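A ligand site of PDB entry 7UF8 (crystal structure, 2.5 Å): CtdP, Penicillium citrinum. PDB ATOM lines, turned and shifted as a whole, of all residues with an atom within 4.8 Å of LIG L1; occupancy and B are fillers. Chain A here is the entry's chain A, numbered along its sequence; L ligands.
The side-chain carboxylate (OD1) of Asp 59 lies close to a nitrogen (N4) of LIG L1, 3.4 Å away. Gly 12 touches LIG L1. Gly 15 touches LIG L1. N of Gly 60 touches C9 of LIG L1, 3.6 Å away. Phe 97 touches LIG L1 (CE2 to N2, 3.1 Å). NE2 of Gln 118 touches C20 of LIG L1, at 3.3 Å. Val 133 touches LIG L1 (CG2 to O13, 3.2 Å). Lys 137 touches LIG L1 (NZ to O11, 3.9 Å). Ala 158 touches LIG L1. Ser 159 touches LIG L1 (O to C19, 3.4 Å). Hydrophobic or aromatic side chains that line LIG L1: Tyr 82, Phe 97, Val 133, Ala 158 and Tyr 161. Of the 30 residues printed, 23 come within 4 Å of LIG L1. Along chain A the residues within 4 Å of LIG L1 span positions 12 to 340.
N of Asp 39 sits at hydrogen-bond distance from OG1 of Thr 37 (3.3 Å). NZ of Lys 137 sits at hydrogen-bond distance from OD1 of Asn 80 (3.0 Å). N of Tyr 161 lies within hydrogen-bond range of OD1 of Asn 164 (3.0 Å). The side-chain hydroxyl of Tyr 161 sits at hydrogen-bond distance from the side-chain amide nitrogen of Gln 17, 2.9 Å away. NE2 of Gln 17 sits close to ND2 of Asn 79, at 3.3 Å. NZ of Lys 137 lies within hydrogen-bond range of OD1 of Asn 79, 3.0 Å away. O of Ser 340 lies within hydrogen-bond range of NE2 of Gln 16. The backbone carbonyl oxygen (O) of Ala 158 lies within hydrogen-bond range of the side-chain amide nitrogen (NE2) of Gln 118 (3.1 Å).
OG1 of Thr 37 sits at hydrogen-bond distance from O17 of LIG L1. OG1 of Thr 14 is in hydrogen-bond range of O5 of LIG L1 (2.7 Å). The side-chain amide oxygen (OD1) of Asn 80 lies within hydrogen-bond range of an oxygen (O12) of LIG L1 (2.8 Å). The side-chain amide oxygen of Asn 61 lies within hydrogen-bond range of a nitrogen (N3) of LIG L1. The side-chain hydroxyl (OH) of Tyr 161 lies close to an oxygen (O8) of LIG L1, 3.5 Å away. The side-chain amide nitrogen (ND2) of Asn 79 lies within hydrogen-bond range of an oxygen (O9) of LIG L1. OD1 of Asn 164 sits at hydrogen-bond distance from N7 of LIG L1, 3.0 Å away. The side-chain hydroxyl (OG) of Ser 340 lies within hydrogen-bond range of an oxygen (O2) of LIG L1 (3.1 Å). An oxygen (O8) of LIG L1 lies within hydrogen-bond range of the side-chain hydroxyl of Tyr 82 (3.1 Å). NE of Arg 38 is in salt-bridge range of O15 of LIG L1, at 3.3 Å. O8 of LIG L1 sits at hydrogen-bond distance from NE2 of Gln 16, at 3.2 Å. O of Gly 81 is in hydrogen-bond range of O12 of LIG L1, 3.3 Å away. The backbone NH (N) of Gln 17 lies within hydrogen-bond range of an oxygen (O9) of LIG L1, 3.5 Å away. The side-chain amide nitrogen (NE2) of Gln 17 lies within hydrogen-bond range of an oxygen (O11) of LIG L1 (3.5 Å).
An oxygen (O13) of LIG L1 is in hydrogen-bond range of an oxygen (O1) of LG2 L2 (3.4 Å).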
ATOM      1  N   GLY A  12     -13.668  -8.043 -23.419  1.00  0.00           N
ATOM      2  CA  GLY A  12     -13.006  -8.763 -24.486  1.00  0.00           C
ATOM      3  C   GLY A  12     -12.751 -10.214 -24.161  1.00  0.00           C
ATOM      4  O   GLY A  12     -11.772 -10.797 -24.661  1.00  0.00           O
ATOM      5  N   ALA A  13     -13.603 -10.824 -23.351  1.00  0.00           N
ATOM      6  CA  ALA A  13     -13.391 -12.209 -22.942  1.00  0.00           C
ATOM      7  C   ALA A  13     -13.390 -13.156 -24.137  1.00  0.00           C
ATOM      8  O   ALA A  13     -12.735 -14.208 -24.095  1.00  0.00           O
ATOM      9  CB  ALA A  13     -14.455 -12.641 -21.942  1.00  0.00           C
ATOM     10  N   THR A  14     -14.101 -12.813 -25.206  1.00  0.00           N
ATOM     11  CA  THR A  14     -14.037 -13.613 -26.422  1.00  0.00           C
ATOM     12  C   THR A  14     -12.759 -13.346 -27.217  1.00  0.00           C
ATOM     13  O   THR A  14     -12.495 -14.053 -28.186  1.00  0.00           O
ATOM     14  CB  THR A  14     -15.245 -13.340 -27.334  1.00  0.00           C
ATOM     15  OG1 THR A  14     -15.130 -12.030 -27.907  1.00  0.00           O
ATOM     16  CG2 THR A  14     -16.540 -13.433 -26.542  1.00  0.00           C
ATOM     17  N   GLY A  15     -11.963 -12.360 -26.815  1.00  0.00           N
ATOM     18  CA  GLY A  15     -10.746 -12.016 -27.513  1.00  0.00           C
ATOM     19  C   GLY A  15      -9.522 -12.614 -26.854  1.00  0.00           C
ATOM     20  O   GLY A  15      -9.598 -13.424 -25.930  1.00  0.00           O
ATOM     21  N   GLN A  16      -8.353 -12.199 -27.349  1.00  0.00           N
ATOM     22  CA  GLN A  16      -7.107 -12.823 -26.922  1.00  0.00           C
ATOM     23  C   GLN A  16      -6.780 -12.461 -25.474  1.00  0.00           C
ATOM     24  O   GLN A  16      -6.647 -13.340 -24.614  1.00  0.00           O
ATOM     25  CB  GLN A  16      -5.994 -12.400 -27.887  1.00  0.00           C
ATOM     26  CG  GLN A  16      -6.023 -13.195 -29.207  1.00  0.00           C
ATOM     27  CD  GLN A  16      -5.227 -12.552 -30.325  1.00  0.00           C
ATOM     28  OE1 GLN A  16      -4.179 -13.068 -30.735  1.00  0.00           O
ATOM     29  NE2 GLN A  16      -5.726 -11.447 -30.856  1.00  0.00           N
ATOM     30  N   GLN A  17      -6.696 -11.157 -25.171  1.00  0.00           N
ATOM     31  CA  GLN A  17      -6.321 -10.752 -23.822  1.00  0.00           C
ATOM     32  C   GLN A  17      -7.359 -11.184 -22.804  1.00  0.00           C
ATOM     33  O   GLN A  17      -7.058 -11.951 -21.879  1.00  0.00           O
ATOM     34  CB  GLN A  17      -6.128  -9.237 -23.774  1.00  0.00           C
ATOM     35  CG  GLN A  17      -4.755  -8.764 -24.194  1.00  0.00           C
ATOM     36  CD  GLN A  17      -4.627  -7.259 -24.168  1.00  0.00           C
ATOM     37  OE1 GLN A  17      -4.849  -6.620 -23.135  1.00  0.00           O
ATOM     38  NE2 GLN A  17      -4.278  -6.669 -25.302  1.00  0.00           N
ATOM     39  N   GLY A  18      -8.607 -10.717 -22.969  1.00  0.00           N
ATOM     40  CA  GLY A  18      -9.645 -11.066 -22.033  1.00  0.00           C
ATOM     41  C   GLY A  18      -9.891 -12.566 -21.958  1.00  0.00           C
ATOM     42  O   GLY A  18     -10.261 -13.080 -20.896  1.00  0.00           O
ATOM     43  N   ILE A  36     -17.850 -10.276 -20.551  1.00  0.00           N
ATOM     44  CA  ILE A  36     -18.694  -9.248 -21.149  1.00  0.00           C
ATOM     45  C   ILE A  36     -18.516  -9.313 -22.649  1.00  0.00           C
ATOM     46  O   ILE A  36     -17.385  -9.374 -23.148  1.00  0.00           O
ATOM     47  CB  ILE A  36     -18.358  -7.841 -20.611  1.00  0.00           C
ATOM     48  CG1 ILE A  36     -18.420  -7.845 -19.079  1.00  0.00           C
ATOM     49  CG2 ILE A  36     -19.317  -6.810 -21.191  1.00  0.00           C
ATOM     50  CD1 ILE A  36     -19.797  -7.503 -18.520  1.00  0.00           C
ATOM     51  N   THR A  37     -19.633  -9.317 -23.376  1.00  0.00           N
ATOM     52  CA  THR A  37     -19.585  -9.411 -24.836  1.00  0.00           C
ATOM     53  C   THR A  37     -20.792  -8.714 -25.440  1.00  0.00           C
ATOM     54  O   THR A  37     -21.814  -8.495 -24.781  1.00  0.00           O
ATOM     55  CB  THR A  37     -19.533 -10.871 -25.296  1.00  0.00           C
ATOM     56  OG1 THR A  37     -19.317 -10.912 -26.707  1.00  0.00           O
ATOM     57  CG2 THR A  37     -20.843 -11.573 -24.955  1.00  0.00           C
ATOM     58  N   ARG A  38     -20.653  -8.367 -26.713  1.00  0.00           N
ATOM     59  CA  ARG A  38     -21.770  -7.823 -27.483  1.00  0.00           C
ATOM     60  C   ARG A  38     -22.717  -8.906 -27.986  1.00  0.00           C
ATOM     61  O   ARG A  38     -23.891  -8.604 -28.244  1.00  0.00           O
ATOM     62  CB  ARG A  38     -21.230  -7.005 -28.665  1.00  0.00           C
ATOM     63  CG  ARG A  38     -20.496  -5.739 -28.268  1.00  0.00           C
ATOM     64  CD  ARG A  38     -19.797  -5.108 -29.456  1.00  0.00           C
ATOM     65  NE  ARG A  38     -18.762  -5.976 -30.019  1.00  0.00           N
ATOM     66  CZ  ARG A  38     -18.024  -5.682 -31.075  1.00  0.00           C
ATOM     67  NH1 ARG A  38     -18.162  -4.536 -31.714  1.00  0.00           N
ATOM     68  NH2 ARG A  38     -17.121  -6.570 -31.498  1.00  0.00           N
ATOM     69  N   ASP A  39     -22.241 -10.143 -28.130  1.00  0.00           N
ATOM     70  CA  ASP A  39     -23.042 -11.207 -28.737  1.00  0.00           C
ATOM     71  C   ASP A  39     -22.793 -12.489 -27.951  1.00  0.00           C
ATOM     72  O   ASP A  39     -21.736 -13.122 -28.091  1.00  0.00           O
ATOM     73  CB  ASP A  39     -22.687 -11.376 -30.203  1.00  0.00           C
ATOM     74  CG  ASP A  39     -23.551 -12.416 -30.890  1.00  0.00           C
ATOM     75  OD1 ASP A  39     -24.682 -12.654 -30.420  1.00  0.00           O
ATOM     76  OD2 ASP A  39     -23.099 -12.990 -31.902  1.00  0.00           O
ATOM     77  N   ASP A  59     -22.735  -3.598 -24.486  1.00  0.00           N
ATOM     78  CA  ASP A  59     -21.902  -2.912 -25.465  1.00  0.00           C
ATOM     79  C   ASP A  59     -21.178  -1.749 -24.798  1.00  0.00           C
ATOM     80  O   ASP A  59     -21.809  -0.937 -24.110  1.00  0.00           O
ATOM     81  CB  ASP A  59     -22.727  -2.409 -26.644  1.00  0.00           C
ATOM     82  CG  ASP A  59     -21.874  -2.028 -27.834  1.00  0.00           C
ATOM     83  OD1 ASP A  59     -21.066  -1.076 -27.709  1.00  0.00           O
ATOM     84  OD2 ASP A  59     -21.998  -2.679 -28.894  1.00  0.00           O
ATOM     85  N   GLY A  60     -19.864  -1.672 -24.998  1.00  0.00           N
ATOM     86  CA  GLY A  60     -19.075  -0.622 -24.364  1.00  0.00           C
ATOM     87  C   GLY A  60     -19.462   0.779 -24.787  1.00  0.00           C
ATOM     88  O   GLY A  60     -19.276   1.737 -24.023  1.00  0.00           O
ATOM     89  N   ASN A  61     -20.001   0.941 -25.989  1.00  0.00           N
ATOM     90  CA  ASN A  61     -20.421   2.249 -26.477  1.00  0.00           C
ATOM     91  C   ASN A  61     -21.730   2.715 -25.849  1.00  0.00           C
ATOM     92  O   ASN A  61     -22.162   3.846 -26.110  1.00  0.00           O
ATOM     93  CB  ASN A  61     -20.550   2.245 -27.997  1.00  0.00           C
ATOM     94  CG  ASN A  61     -19.279   1.802 -28.687  1.00  0.00           C
ATOM     95  OD1 ASN A  61     -19.200   0.691 -29.220  1.00  0.00           O
ATOM     96  ND2 ASN A  61     -18.270   2.668 -28.681  1.00  0.00           N
ATOM     97  N   ASN A  79     -10.076  -3.844 -21.765  1.00  0.00           N
ATOM     98  CA  ASN A  79      -9.277  -3.842 -22.991  1.00  0.00           C
ATOM     99  C   ASN A  79     -10.126  -3.231 -24.107  1.00  0.00           C
ATOM    100  O   ASN A  79     -11.338  -3.048 -23.955  1.00  0.00           O
ATOM    101  CB  ASN A  79      -8.824  -5.265 -23.359  1.00  0.00           C
ATOM    102  CG  ASN A  79      -7.688  -5.275 -24.356  1.00  0.00           C
ATOM    103  OD1 ASN A  79      -6.947  -4.302 -24.474  1.00  0.00           O
ATOM    104  ND2 ASN A  79      -7.534  -6.383 -25.069  1.00  0.00           N
ATOM    105  N   ASN A  80      -9.470  -2.896 -25.207  1.00  0.00           N
ATOM    106  CA  ASN A  80     -10.133  -2.329 -26.377  1.00  0.00           C
ATOM    107  C   ASN A  80      -9.861  -3.222 -27.598  1.00  0.00           C
ATOM    108  O   ASN A  80      -9.325  -4.327 -27.471  1.00  0.00           O
ATOM    109  CB  ASN A  80      -9.690  -0.877 -26.597  1.00  0.00           C
ATOM    110  CG  ASN A  80      -8.293  -0.774 -27.180  1.00  0.00           C
ATOM    111  OD1 ASN A  80      -7.502  -1.716 -27.120  1.00  0.00           O
ATOM    112  ND2 ASN A  80      -7.975   0.397 -27.738  1.00  0.00           N
ATOM    113  N   GLY A  81     -10.233  -2.725 -28.785  1.00  0.00           N
ATOM    114  CA  GLY A  81     -10.143  -3.499 -30.005  1.00  0.00           C
ATOM    115  C   GLY A  81      -9.160  -2.901 -30.993  1.00  0.00           C
ATOM    116  O   GLY A  81      -8.700  -1.761 -30.848  1.00  0.00           O
ATOM    117  N   TYR A  82      -8.829  -3.696 -32.018  1.00  0.00           N
ATOM    118  CA  TYR A  82      -7.863  -3.269 -33.027  1.00  0.00           C
ATOM    119  C   TYR A  82      -8.415  -2.188 -33.941  1.00  0.00           C
ATOM    120  O   TYR A  82      -7.629  -1.500 -34.609  1.00  0.00           O
ATOM    121  CB  TYR A  82      -7.439  -4.468 -33.871  1.00  0.00           C
ATOM    122  CG  TYR A  82      -6.546  -5.452 -33.150  1.00  0.00           C
ATOM    123  CD1 TYR A  82      -5.193  -5.199 -32.968  1.00  0.00           C
ATOM    124  CD2 TYR A  82      -7.058  -6.644 -32.657  1.00  0.00           C
ATOM    125  CE1 TYR A  82      -4.372  -6.106 -32.319  1.00  0.00           C
ATOM    126  CE2 TYR A  82      -6.245  -7.561 -32.002  1.00  0.00           C
ATOM    127  CZ  TYR A  82      -4.897  -7.282 -31.835  1.00  0.00           C
ATOM    128  OH  TYR A  82      -4.090  -8.186 -31.183  1.00  0.00           O
ATOM    129  N   PHE A  97     -14.454   2.434 -26.837  1.00  0.00           N
ATOM    130  CA  PHE A  97     -15.373   1.672 -25.984  1.00  0.00           C
ATOM    131  C   PHE A  97     -14.684   1.172 -24.718  1.00  0.00           C
ATOM    132  O   PHE A  97     -15.326   1.067 -23.669  1.00  0.00           O
ATOM    133  CB  PHE A  97     -16.031   0.521 -26.776  1.00  0.00           C
ATOM    134  CG  PHE A  97     -15.143  -0.685 -26.957  1.00  0.00           C
ATOM    135  CD1 PHE A  97     -15.118  -1.687 -25.996  1.00  0.00           C
ATOM    136  CD2 PHE A  97     -14.381  -0.843 -28.094  1.00  0.00           C
ATOM    137  CE1 PHE A  97     -14.309  -2.794 -26.154  1.00  0.00           C
ATOM    138  CE2 PHE A  97     -13.576  -1.955 -28.268  1.00  0.00           C
ATOM    139  CZ  PHE A  97     -13.544  -2.929 -27.300  1.00  0.00           C
ATOM    140  N   GLN A 118      -1.027   1.283 -22.963  1.00  0.00           N
ATOM    141  CA  GLN A 118       0.183   1.519 -23.734  1.00  0.00           C
ATOM    142  C   GLN A 118       0.591   2.955 -23.487  1.00  0.00           C
ATOM    143  O   GLN A 118      -0.242   3.779 -23.091  1.00  0.00           O
ATOM    144  CB  GLN A 118      -0.029   1.265 -25.228  1.00  0.00           C
ATOM    145  CG  GLN A 118      -0.304  -0.185 -25.602  1.00  0.00           C
ATOM    146  CD  GLN A 118       0.919  -1.071 -25.428  1.00  0.00           C
ATOM    147  OE1 GLN A 118       2.051  -0.589 -25.403  1.00  0.00           O
ATOM    148  NE2 GLN A 118       0.689  -2.368 -25.330  1.00  0.00           N
ATOM    149  N   VAL A 133      -3.220   4.186 -31.823  1.00  0.00           N
ATOM    150  CA  VAL A 133      -3.324   2.796 -31.369  1.00  0.00           C
ATOM    151  C   VAL A 133      -2.812   2.640 -29.940  1.00  0.00           C
ATOM    152  O   VAL A 133      -3.325   1.817 -29.170  1.00  0.00           O
ATOM    153  CB  VAL A 133      -2.586   1.856 -32.344  1.00  0.00           C
ATOM    154  CG1 VAL A 133      -1.081   2.123 -32.299  1.00  0.00           C
ATOM    155  CG2 VAL A 133      -2.887   0.400 -32.035  1.00  0.00           C
ATOM    156  N   LYS A 137      -5.280   4.094 -25.461  1.00  0.00           N
ATOM    157  CA  LYS A 137      -5.218   3.248 -24.256  1.00  0.00           C
ATOM    158  C   LYS A 137      -4.587   4.141 -23.190  1.00  0.00           C
ATOM    159  O   LYS A 137      -5.042   4.117 -22.101  1.00  0.00           O
ATOM    160  CB  LYS A 137      -4.443   1.945 -24.535  1.00  0.00           C
ATOM    161  CG  LYS A 137      -4.834   1.180 -25.817  1.00  0.00           C
ATOM    162  CD  LYS A 137      -3.971  -0.097 -26.117  1.00  0.00           C
ATOM    163  CE  LYS A 137      -4.110  -1.208 -25.058  1.00  0.00           C
ATOM    164  NZ  LYS A 137      -5.542  -1.665 -24.914  1.00  0.00           N
ATOM    165  N   ALA A 158       0.751  -4.915 -22.728  1.00  0.00           N
ATOM    166  CA  ALA A 158       1.059  -6.156 -23.448  1.00  0.00           C
ATOM    167  C   ALA A 158       2.248  -5.971 -24.385  1.00  0.00           C
ATOM    168  O   ALA A 158       2.415  -4.909 -24.995  1.00  0.00           O
ATOM    169  CB  ALA A 158      -0.169  -6.604 -24.241  1.00  0.00           C
ATOM    170  N   SER A 159       3.058  -7.017 -24.489  1.00  0.00           N
ATOM    171  CA  SER A 159       4.163  -7.051 -25.436  1.00  0.00           C
ATOM    172  C   SER A 159       3.672  -7.482 -26.820  1.00  0.00           C
ATOM    173  O   SER A 159       2.482  -7.679 -27.055  1.00  0.00           O
ATOM    174  CB  SER A 159       5.226  -8.026 -24.937  1.00  0.00           C
ATOM    175  OG  SER A 159       5.960  -7.454 -23.876  1.00  0.00           O
ATOM    176  N   TRP A 160       4.608  -7.635 -27.759  1.00  0.00           N
ATOM    177  CA  TRP A 160       4.285  -8.321 -28.999  1.00  0.00           C
ATOM    178  C   TRP A 160       3.739  -9.696 -28.640  1.00  0.00           C
ATOM    179  O   TRP A 160       4.381 -10.437 -27.876  1.00  0.00           O
ATOM    180  CB  TRP A 160       5.530  -8.492 -29.878  1.00  0.00           C
ATOM    181  CG  TRP A 160       6.100  -7.253 -30.499  1.00  0.00           C
ATOM    182  CD1 TRP A 160       6.962  -6.368 -29.919  1.00  0.00           C
ATOM    183  CD2 TRP A 160       5.878  -6.768 -31.837  1.00  0.00           C
ATOM    184  NE1 TRP A 160       7.278  -5.364 -30.796  1.00  0.00           N
ATOM    185  CE2 TRP A 160       6.622  -5.579 -31.979  1.00  0.00           C
ATOM    186  CE3 TRP A 160       5.122  -7.214 -32.920  1.00  0.00           C
ATOM    187  CZ2 TRP A 160       6.627  -4.831 -33.154  1.00  0.00           C
ATOM    188  CZ3 TRP A 160       5.132  -6.478 -34.091  1.00  0.00           C
ATOM    189  CH2 TRP A 160       5.874  -5.296 -34.198  1.00  0.00           C
ATOM    190  N   TYR A 161       2.574 -10.064 -29.162  1.00  0.00           N
ATOM    191  CA  TYR A 161       2.134 -11.435 -28.972  1.00  0.00           C
ATOM    192  C   TYR A 161       3.034 -12.334 -29.804  1.00  0.00           C
ATOM    193  O   TYR A 161       3.372 -12.003 -30.948  1.00  0.00           O
ATOM    194  CB  TYR A 161       0.682 -11.681 -29.397  1.00  0.00           C
ATOM    195  CG  TYR A 161      -0.367 -10.723 -28.889  1.00  0.00           C
ATOM    196  CD1 TYR A 161      -0.067  -9.750 -27.945  1.00  0.00           C
ATOM    197  CD2 TYR A 161      -1.669 -10.792 -29.369  1.00  0.00           C
ATOM    198  CE1 TYR A 161      -1.030  -8.869 -27.516  1.00  0.00           C
ATOM    199  CE2 TYR A 161      -2.639  -9.921 -28.934  1.00  0.00           C
ATOM    200  CZ  TYR A 161      -2.323  -8.960 -28.003  1.00  0.00           C
ATOM    201  OH  TYR A 161      -3.288  -8.088 -27.575  1.00  0.00           O
ATOM    202  N   ASN A 164       1.134 -13.006 -32.764  1.00  0.00           N
ATOM    203  CA  ASN A 164       1.177 -12.185 -33.969  1.00  0.00           C
ATOM    204  C   ASN A 164       1.526 -13.023 -35.193  1.00  0.00           C
ATOM    205  O   ASN A 164       1.149 -12.658 -36.304  1.00  0.00           O
ATOM    206  CB  ASN A 164       2.189 -11.046 -33.823  1.00  0.00           C
ATOM    207  CG  ASN A 164       1.647  -9.857 -33.039  1.00  0.00           C
ATOM    208  OD1 ASN A 164       2.232  -9.456 -32.032  1.00  0.00           O
ATOM    209  ND2 ASN A 164       0.544  -9.292 -33.502  1.00  0.00           N
ATOM    210  N   ILE A 167      -1.670 -13.836 -36.700  1.00  0.00           N
ATOM    211  CA  ILE A 167      -2.422 -12.698 -37.237  1.00  0.00           C
ATOM    212  C   ILE A 167      -1.990 -12.540 -38.692  1.00  0.00           C
ATOM    213  O   ILE A 167      -0.796 -12.361 -38.973  1.00  0.00           O
ATOM    214  CB  ILE A 167      -2.166 -11.420 -36.419  1.00  0.00           C
ATOM    215  CG1 ILE A 167      -2.926 -11.507 -35.097  1.00  0.00           C
ATOM    216  CG2 ILE A 167      -2.615 -10.202 -37.216  1.00  0.00           C
ATOM    217  CD1 ILE A 167      -2.512 -10.474 -34.079  1.00  0.00           C
ATOM    218  N   TYR A 269      -2.418   1.892 -41.553  1.00  0.00           N
ATOM    219  CA  TYR A 269      -1.955   1.256 -40.320  1.00  0.00           C
ATOM    220  C   TYR A 269      -0.451   1.040 -40.375  1.00  0.00           C
ATOM    221  O   TYR A 269       0.228   1.115 -39.344  1.00  0.00           O
ATOM    222  CB  TYR A 269      -2.679  -0.076 -40.086  1.00  0.00           C
ATOM    223  CG  TYR A 269      -2.804  -0.472 -38.621  1.00  0.00           C
ATOM    224  CD1 TYR A 269      -1.762  -1.099 -37.959  1.00  0.00           C
ATOM    225  CD2 TYR A 269      -3.964  -0.188 -37.910  1.00  0.00           C
ATOM    226  CE1 TYR A 269      -1.871  -1.438 -36.615  1.00  0.00           C
ATOM    227  CE2 TYR A 269      -4.086  -0.525 -36.563  1.00  0.00           C
ATOM    228  CZ  TYR A 269      -3.029  -1.161 -35.927  1.00  0.00           C
ATOM    229  OH  TYR A 269      -3.142  -1.506 -34.599  1.00  0.00           O
ATOM    230  N   SER A 340      -7.533 -12.393 -34.687  1.00  0.00           N
ATOM    231  CA  SER A 340      -7.917 -10.989 -34.763  1.00  0.00           C
ATOM    232  C   SER A 340      -6.704 -10.088 -34.585  1.00  0.00           C
ATOM    233  O   SER A 340      -5.890 -10.302 -33.682  1.00  0.00           O
ATOM    234  CB  SER A 340      -8.975 -10.667 -33.694  1.00  0.00           C
ATOM    235  OG  SER A 340      -9.346  -9.306 -33.738  1.00  0.00           O
HETATM  236  P1  LIG L   1      -9.508  -8.364 -30.221  1.00  0.00           P
HETATM  237  O1  LIG L   1      -8.912  -9.705 -30.507  1.00  0.00           O
HETATM  238  O2  LIG L   1      -9.906  -7.456 -31.330  1.00  0.00           O
HETATM  239  O3  LIG L   1     -10.753  -8.546 -29.238  1.00  0.00           O
HETATM  240  C1  LIG L   1     -11.676  -7.426 -29.149  1.00  0.00           C
HETATM  241  C2  LIG L   1     -12.741  -7.702 -28.092  1.00  0.00           C
HETATM  242  O4  LIG L   1     -13.400  -6.452 -27.806  1.00  0.00           O
HETATM  243  C3  LIG L   1     -13.875  -8.689 -28.489  1.00  0.00           C
HETATM  244  O5  LIG L   1     -14.301  -9.531 -27.412  1.00  0.00           O
HETATM  245  C4  LIG L   1     -14.985  -7.752 -28.999  1.00  0.00           C
HETATM  246  O6  LIG L   1     -16.378  -8.077 -28.832  1.00  0.00           O
HETATM  247  C5  LIG L   1     -14.763  -6.526 -28.109  1.00  0.00           C
HETATM  248  N1  LIG L   1     -15.182  -5.293 -28.773  1.00  0.00           N
HETATM  249  C6  LIG L   1     -14.702  -4.750 -29.939  1.00  0.00           C
HETATM  250  N2  LIG L   1     -15.308  -3.642 -30.276  1.00  0.00           N
HETATM  251  C7  LIG L   1     -16.245  -3.451 -29.274  1.00  0.00           C
HETATM  252  C8  LIG L   1     -17.207  -2.439 -29.046  1.00  0.00           C
HETATM  253  N3  LIG L   1     -17.378  -1.404 -29.851  1.00  0.00           N
HETATM  254  N4  LIG L   1     -17.970  -2.549 -27.936  1.00  0.00           N
HETATM  255  C9  LIG L   1     -17.782  -3.608 -27.133  1.00  0.00           C
HETATM  256  N5  LIG L   1     -16.929  -4.608 -27.253  1.00  0.00           N
HETATM  257  C10 LIG L   1     -16.178  -4.467 -28.345  1.00  0.00           C
HETATM  258  O7  LIG L   1      -8.487  -7.546 -29.298  1.00  0.00           O
HETATM  259  P2  LIG L   1      -7.258  -7.955 -28.367  1.00  0.00           P
HETATM  260  O8  LIG L   1      -6.297  -8.814 -29.116  1.00  0.00           O
HETATM  261  O9  LIG L   1      -7.844  -8.523 -27.118  1.00  0.00           O
HETATM  262  O10 LIG L   1      -6.614  -6.512 -28.086  1.00  0.00           O
HETATM  263  C11 LIG L   1      -6.159  -5.634 -29.165  1.00  0.00           C
HETATM  264  C12 LIG L   1      -5.907  -4.221 -28.650  1.00  0.00           C
HETATM  265  O11 LIG L   1      -4.795  -4.249 -27.732  1.00  0.00           O
HETATM  266  C13 LIG L   1      -5.510  -3.174 -29.712  1.00  0.00           C
HETATM  267  O12 LIG L   1      -5.772  -1.804 -29.370  1.00  0.00           O
HETATM  268  C14 LIG L   1      -3.997  -3.401 -29.823  1.00  0.00           C
HETATM  269  O13 LIG L   1      -3.337  -2.269 -30.398  1.00  0.00           O
HETATM  270  C15 LIG L   1      -3.630  -3.669 -28.344  1.00  0.00           C
HETATM  271  N6  LIG L   1      -2.483  -4.627 -28.141  1.00  0.00           N
HETATM  272  C16 LIG L   1      -2.283  -5.708 -28.980  1.00  0.00           C
HETATM  273  C17 LIG L   1      -0.990  -6.163 -29.187  1.00  0.00           C
HETATM  274  C18 LIG L   1      -0.687  -7.011 -30.407  1.00  0.00           C
HETATM  275  O14 LIG L   1      -1.301  -6.807 -31.438  1.00  0.00           O
HETATM  276  N7  LIG L   1       0.288  -7.901 -30.360  1.00  0.00           N
HETATM  277  C19 LIG L   1       0.009  -5.787 -28.292  1.00  0.00           C
HETATM  278  C20 LIG L   1      -0.285  -4.863 -27.319  1.00  0.00           C
HETATM  279  C21 LIG L   1      -1.604  -4.480 -27.135  1.00  0.00           C
HETATM  280  P3  LIG L   1     -17.058  -9.464 -29.271  1.00  0.00           P
HETATM  281  O15 LIG L   1     -18.436  -9.299 -29.854  1.00  0.00           O
HETATM  282  O16 LIG L   1     -16.108 -10.188 -30.218  1.00  0.00           O
HETATM  283  O17 LIG L   1     -17.096 -10.013 -27.875  1.00  0.00           O
HETATM  284  C1  LG2 L   2       0.317  -6.767 -37.418  1.00  0.00           C
HETATM  285  C2  LG2 L   2       0.156  -5.657 -38.285  1.00  0.00           C
HETATM  286  C3  LG2 L   2       0.413  -4.382 -37.823  1.00  0.00           C
HETATM  287  C4  LG2 L   2       0.840  -4.250 -36.489  1.00  0.00           C
HETATM  288  C5  LG2 L   2       1.012  -5.326 -35.599  1.00  0.00           C
HETATM  289  C6  LG2 L   2       2.638  -2.999 -32.278  1.00  0.00           C
HETATM  290  C7  LG2 L   2       1.453  -4.726 -34.340  1.00  0.00           C
HETATM  291  C8  LG2 L   2       1.528  -3.363 -34.508  1.00  0.00           C
HETATM  292  C9  LG2 L   2       0.612  -1.447 -33.177  1.00  0.00           C
HETATM  293  C10 LG2 L   2       1.908  -4.318 -31.825  1.00  0.00           C
HETATM  294  C11 LG2 L   2       1.793  -5.333 -33.059  1.00  0.00           C
HETATM  295  C12 LG2 L   2       2.997  -1.253 -34.167  1.00  0.00           C
HETATM  296  C13 LG2 L   2       2.999  -2.102 -30.986  1.00  0.00           C
HETATM  297  C14 LG2 L   2       2.366  -2.811 -29.717  1.00  0.00           C
HETATM  298  C15 LG2 L   2       2.822  -5.038 -30.718  1.00  0.00           C
HETATM  299  C16 LG2 L   2       2.659  -2.280 -28.322  1.00  0.00           C
HETATM  300  C17 LG2 L   2       3.998  -2.984 -27.783  1.00  0.00           C
HETATM  301  C18 LG2 L   2       4.244  -4.087 -28.849  1.00  0.00           C
HETATM  302  C19 LG2 L   2       0.875  -2.859 -30.172  1.00  0.00           C
HETATM  303  C20 LG2 L   2       1.927  -2.280 -33.511  1.00  0.00           C
HETATM  304  C21 LG2 L   2       0.747  -6.600 -36.104  1.00  0.00           C
HETATM  305  N1  LG2 L   2       1.155  -3.110 -35.783  1.00  0.00           N
HETATM  306  N2  LG2 L   2       2.878  -4.195 -29.500  1.00  0.00           N
HETATM  307  N3  LG2 L   2       0.692  -3.953 -31.039  1.00  0.00           N
HETATM  308  O1  LG2 L   2      -0.022  -2.115 -29.862  1.00  0.00           O
